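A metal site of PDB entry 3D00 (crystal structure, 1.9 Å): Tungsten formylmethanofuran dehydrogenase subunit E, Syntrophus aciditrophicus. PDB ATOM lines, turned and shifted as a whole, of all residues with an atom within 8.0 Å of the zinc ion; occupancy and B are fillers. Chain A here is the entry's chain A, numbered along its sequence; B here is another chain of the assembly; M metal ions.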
ATOM      1  N   LEU A 165       9.088  24.846 -21.435  1.00  0.00           N
ATOM      2  CA  LEU A 165       8.372  26.060 -21.888  1.00  0.00           C
ATOM      3  C   LEU A 165       7.859  25.939 -23.326  1.00  0.00           C
ATOM      4  O   LEU A 165       8.642  25.717 -24.253  1.00  0.00           O
ATOM      5  CB  LEU A 165       9.275  27.303 -21.787  1.00  0.00           C
ATOM      6  CG  LEU A 165       8.643  28.690 -22.001  1.00  0.00           C
ATOM      7  CD1 LEU A 165       7.523  28.927 -21.001  1.00  0.00           C
ATOM      8  CD2 LEU A 165       9.667  29.849 -21.946  1.00  0.00           C
ATOM      9  N   CYS A 166       6.554  26.095 -23.519  1.00  0.00           N
ATOM     10  CA  CYS A 166       5.995  26.007 -24.872  1.00  0.00           C
ATOM     11  C   CYS A 166       6.476  27.189 -25.670  1.00  0.00           C
ATOM     12  O   CYS A 166       6.275  28.314 -25.243  1.00  0.00           O
ATOM     13  CB  CYS A 166       4.489  25.976 -24.845  1.00  0.00           C
ATOM     14  SG  CYS A 166       3.781  25.876 -26.489  1.00  0.00           S
ATOM     15  N   PRO A 167       7.113  26.946 -26.825  1.00  0.00           N
ATOM     16  CA  PRO A 167       7.625  28.059 -27.614  1.00  0.00           C
ATOM     17  C   PRO A 167       6.552  28.950 -28.174  1.00  0.00           C
ATOM     18  O   PRO A 167       6.810  30.101 -28.482  1.00  0.00           O
ATOM     19  CB  PRO A 167       8.350  27.376 -28.768  1.00  0.00           C
ATOM     20  CG  PRO A 167       7.853  25.998 -28.813  1.00  0.00           C
ATOM     21  CD  PRO A 167       7.407  25.635 -27.455  1.00  0.00           C
ATOM     22  N   GLN A 168       5.356  28.403 -28.365  1.00  0.00           N
ATOM     23  CA  GLN A 168       4.301  29.149 -29.009  1.00  0.00           C
ATOM     24  C   GLN A 168       3.556  30.058 -28.040  1.00  0.00           C
ATOM     25  O   GLN A 168       3.335  31.242 -28.350  1.00  0.00           O
ATOM     26  CB  GLN A 168       3.347  28.195 -29.732  1.00  0.00           C
ATOM     27  CG  GLN A 168       2.458  28.921 -30.684  1.00  0.00           C
ATOM     28  CD  GLN A 168       1.364  28.072 -31.216  1.00  0.00           C
ATOM     29  OE1 GLN A 168       1.604  26.975 -31.747  1.00  0.00           O
ATOM     30  NE2 GLN A 168       0.141  28.556 -31.069  1.00  0.00           N
ATOM     31  N   CYS A 169       3.178  29.547 -26.861  1.00  0.00           N
ATOM     32  CA  CYS A 169       2.430  30.365 -25.893  1.00  0.00           C
ATOM     33  C   CYS A 169       3.240  30.783 -24.693  1.00  0.00           C
ATOM     34  O   CYS A 169       2.768  31.599 -23.903  1.00  0.00           O
ATOM     35  CB  CYS A 169       1.170  29.630 -25.420  1.00  0.00           C
ATOM     36  SG  CYS A 169       1.499  28.269 -24.294  1.00  0.00           S
ATOM     37  N   ARG A 170       4.439  30.228 -24.568  1.00  0.00           N
ATOM     38  CA  ARG A 170       5.369  30.488 -23.462  1.00  0.00           C
ATOM     39  C   ARG A 170       4.739  30.271 -22.113  1.00  0.00           C
ATOM     40  O   ARG A 170       4.891  31.102 -21.200  1.00  0.00           O
ATOM     41  CB  ARG A 170       5.999  31.871 -23.579  1.00  0.00           C
ATOM     42  CG  ARG A 170       6.808  32.053 -24.858  1.00  0.00           C
ATOM     43  CD  ARG A 170       7.538  33.412 -24.893  1.00  0.00           C
ATOM     44  NE  ARG A 170       8.125  33.851 -23.611  1.00  0.00           N
ATOM     45  CZ  ARG A 170       9.314  33.476 -23.143  1.00  0.00           C
ATOM     46  NH1 ARG A 170      10.093  32.636 -23.818  1.00  0.00           N
ATOM     47  NH2 ARG A 170       9.719  33.937 -21.958  1.00  0.00           N
ATOM     48  N   GLU A 171       4.048  29.143 -21.990  1.00  0.00           N
ATOM     49  CA  GLU A 171       3.607  28.642 -20.715  1.00  0.00           C
ATOM     50  C   GLU A 171       4.325  27.329 -20.394  1.00  0.00           C
ATOM     51  O   GLU A 171       4.761  26.613 -21.286  1.00  0.00           O
ATOM     52  CB  GLU A 171       2.091  28.492 -20.711  1.00  0.00           C
ATOM     53  CG  GLU A 171       1.371  29.842 -20.463  1.00  0.00           C
ATOM     54  CD  GLU A 171      -0.114  29.790 -20.646  1.00  0.00           C
ATOM     55  OE1 GLU A 171      -0.756  28.965 -19.949  1.00  0.00           O
ATOM     56  OE2 GLU A 171      -0.636  30.571 -21.484  1.00  0.00           O
ATOM     57  N   ALA A 172       4.447  27.028 -19.111  1.00  0.00           N
ATOM     58  CA  ALA A 172       5.047  25.786 -18.674  1.00  0.00           C
ATOM     59  C   ALA A 172       4.089  24.606 -18.883  1.00  0.00           C
ATOM     60  O   ALA A 172       2.874  24.705 -18.686  1.00  0.00           O
ATOM     61  CB  ALA A 172       5.480  25.878 -17.208  1.00  0.00           C
ATOM     62  N   TYR A 173       4.661  23.493 -19.328  1.00  0.00           N
ATOM     63  CA  TYR A 173       3.917  22.261 -19.577  1.00  0.00           C
ATOM     64  C   TYR A 173       4.863  21.030 -19.438  1.00  0.00           C
ATOM     65  O   TYR A 173       6.075  21.167 -19.441  1.00  0.00           O
ATOM     66  CB  TYR A 173       3.210  22.318 -20.960  1.00  0.00           C
ATOM     67  CG  TYR A 173       4.130  22.096 -22.125  1.00  0.00           C
ATOM     68  CD1 TYR A 173       5.015  23.073 -22.539  1.00  0.00           C
ATOM     69  CD2 TYR A 173       4.156  20.875 -22.788  1.00  0.00           C
ATOM     70  CE1 TYR A 173       5.916  22.849 -23.589  1.00  0.00           C
ATOM     71  CE2 TYR A 173       5.049  20.654 -23.858  1.00  0.00           C
ATOM     72  CZ  TYR A 173       5.914  21.652 -24.256  1.00  0.00           C
ATOM     73  OH  TYR A 173       6.815  21.464 -25.313  1.00  0.00           O
ATOM     74  N   GLU A 179       6.425  18.972 -28.496  1.00  0.00           N
ATOM     75  CA  GLU A 179       7.233  20.157 -28.784  1.00  0.00           C
ATOM     76  C   GLU A 179       6.425  21.423 -28.615  1.00  0.00           C
ATOM     77  O   GLU A 179       6.977  22.527 -28.626  1.00  0.00           O
ATOM     78  CB  GLU A 179       7.773  20.129 -30.207  1.00  0.00           C
ATOM     79  CG  GLU A 179       8.174  18.772 -30.752  1.00  0.00           C
ATOM     80  CD  GLU A 179       8.445  18.856 -32.244  1.00  0.00           C
ATOM     81  OE1 GLU A 179       9.345  19.639 -32.633  1.00  0.00           O
ATOM     82  OE2 GLU A 179       7.717  18.184 -33.011  1.00  0.00           O
ATOM     83  N   LEU A 180       5.112  21.274 -28.557  1.00  0.00           N
ATOM     84  CA  LEU A 180       4.252  22.325 -28.054  1.00  0.00           C
ATOM     85  C   LEU A 180       3.399  21.694 -26.987  1.00  0.00           C
ATOM     86  O   LEU A 180       3.364  20.478 -26.798  1.00  0.00           O
ATOM     87  CB  LEU A 180       3.339  22.897 -29.140  1.00  0.00           C
ATOM     88  CG  LEU A 180       3.920  23.436 -30.436  1.00  0.00           C
ATOM     89  CD1 LEU A 180       2.818  23.450 -31.482  1.00  0.00           C
ATOM     90  CD2 LEU A 180       4.540  24.827 -30.263  1.00  0.00           C
ATOM     91  N   CYS A 181       2.724  22.538 -26.241  1.00  0.00           N
ATOM     92  CA  CYS A 181       1.787  22.057 -25.273  1.00  0.00           C
ATOM     93  C   CYS A 181       0.524  21.641 -26.005  1.00  0.00           C
ATOM     94  O   CYS A 181       0.321  21.946 -27.195  1.00  0.00           O
ATOM     95  CB  CYS A 181       1.459  23.126 -24.244  1.00  0.00           C
ATOM     96  SG  CYS A 181       0.457  24.421 -24.917  1.00  0.00           S
ATOM     97  N   LEU A 182      -0.291  20.902 -25.264  1.00  0.00           N
ATOM     98  CA  LEU A 182      -1.471  20.264 -25.818  1.00  0.00           C
ATOM     99  C   LEU A 182      -2.471  21.305 -26.276  1.00  0.00           C
ATOM    100  O   LEU A 182      -3.241  21.070 -27.183  1.00  0.00           O
ATOM    101  CB  LEU A 182      -2.065  19.295 -24.820  1.00  0.00           C
ATOM    102  CG  LEU A 182      -1.308  17.968 -24.577  1.00  0.00           C
ATOM    103  CD1 LEU A 182      -1.898  17.139 -23.431  1.00  0.00           C
ATOM    104  CD2 LEU A 182      -1.205  17.109 -25.872  1.00  0.00           C
ATOM    105  N   SER A 183      -2.457  22.492 -25.666  1.00  0.00           N
ATOM    106  CA  SER A 183      -3.321  23.569 -26.114  1.00  0.00           C
ATOM    107  C   SER A 183      -2.881  24.030 -27.500  1.00  0.00           C
ATOM    108  O   SER A 183      -3.685  24.053 -28.441  1.00  0.00           O
ATOM    109  CB  SER A 183      -3.344  24.733 -25.119  1.00  0.00           C
ATOM    110  OG  SER A 183      -4.221  25.749 -25.569  1.00  0.00           O
ATOM    111  N   CYS A 184      -1.602  24.360 -27.631  1.00  0.00           N
ATOM    112  CA  CYS A 184      -1.039  24.838 -28.898  1.00  0.00           C
ATOM    113  C   CYS A 184      -1.053  23.772 -29.986  1.00  0.00           C
ATOM    114  O   CYS A 184      -1.087  24.091 -31.194  1.00  0.00           O
ATOM    115  CB  CYS A 184       0.373  25.414 -28.653  1.00  0.00           C
ATOM    116  SG  CYS A 184       0.304  27.040 -27.875  1.00  0.00           S
ATOM    117  N   GLN A 185      -1.005  22.509 -29.575  1.00  0.00           N
ATOM    118  CA  GLN A 185      -1.173  21.411 -30.513  1.00  0.00           C
ATOM    119  C   GLN A 185      -2.598  21.388 -31.098  1.00  0.00           C
ATOM    120  O   GLN A 185      -2.798  20.848 -32.152  1.00  0.00           O
ATOM    121  CB  GLN A 185      -0.877  20.063 -29.843  1.00  0.00           C
ATOM    122  CG  GLN A 185       0.583  19.821 -29.525  1.00  0.00           C
ATOM    123  CD  GLN A 185       0.825  18.508 -28.791  1.00  0.00           C
ATOM    124  OE1 GLN A 185       0.127  17.524 -29.021  1.00  0.00           O
ATOM    125  NE2 GLN A 185       1.819  18.490 -27.913  1.00  0.00           N
ATOM    126  N   LEU B  84      -1.713  22.607 -18.230  1.00  0.00           N
ATOM    127  CA  LEU B  84      -1.476  24.031 -18.182  1.00  0.00           C
ATOM    128  C   LEU B  84      -2.177  24.589 -16.934  1.00  0.00           C
ATOM    129  O   LEU B  84      -3.337  24.340 -16.714  1.00  0.00           O
ATOM    130  CB  LEU B  84      -1.994  24.723 -19.437  1.00  0.00           C
ATOM    131  CG  LEU B  84      -1.282  24.319 -20.723  1.00  0.00           C
ATOM    132  CD1 LEU B  84      -1.987  24.927 -21.912  1.00  0.00           C
ATOM    133  CD2 LEU B  84       0.203  24.718 -20.700  1.00  0.00           C
ATOM    134  N   ARG B  99      -9.019  34.483 -19.134  1.00  0.00           N
ATOM    135  CA  ARG B  99      -8.140  33.407 -18.770  1.00  0.00           C
ATOM    136  C   ARG B  99      -7.061  33.944 -17.875  1.00  0.00           C
ATOM    137  O   ARG B  99      -6.484  35.015 -18.153  1.00  0.00           O
ATOM    138  CB  ARG B  99      -7.493  32.845 -20.001  1.00  0.00           C
ATOM    139  CG  ARG B  99      -6.630  31.645 -19.748  1.00  0.00           C
ATOM    140  CD  ARG B  99      -6.100  31.221 -21.115  1.00  0.00           C
ATOM    141  NE  ARG B  99      -5.338  29.998 -21.036  1.00  0.00           N
ATOM    142  CZ  ARG B  99      -4.026  29.934 -21.001  1.00  0.00           C
ATOM    143  NH1 ARG B  99      -3.325  31.032 -21.060  1.00  0.00           N
ATOM    144  NH2 ARG B  99      -3.444  28.749 -20.875  1.00  0.00           N
HETATM  145 ZN    ZN M   1       1.542  26.338 -25.838  1.00  0.00          ZN
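Four residues have an atom within 4 Å of the zinc ion: Cys 166, Cys 169, Cys 181 and Cys 184. The nearest printed residue that does not touch the zinc ion is Gln 168 (4.7 Å).
The zinc ion is bound by SG of Cys 166 (2.4 Å), SG of Cys 181 (2.4 Å), SG of Cys 169 (2.5 Å) and SG of Cys 184 (2.5 Å). The zinc ion has four donor atoms within binding distance.
SG of Cys 166 sits close to N of Gln 168, 3.5 Å away. The backbone carbonyl oxygen (O) of Glu 171 sits at hydrogen-bond distance from the backbone NH (N) of Cys 166, at 2.9 Å. The side-chain sulfur (SG) of Cys 181 sits close to the backbone NH (N) of Ser 183, 3.6 Å away. The side-chain sulfur (SG) of Cys 169 lies close to the backbone NH (N) of Glu 171 (3.5 Å). SG of Cys 184 sits close to NE2 of Gln 168 (3.5 Å).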
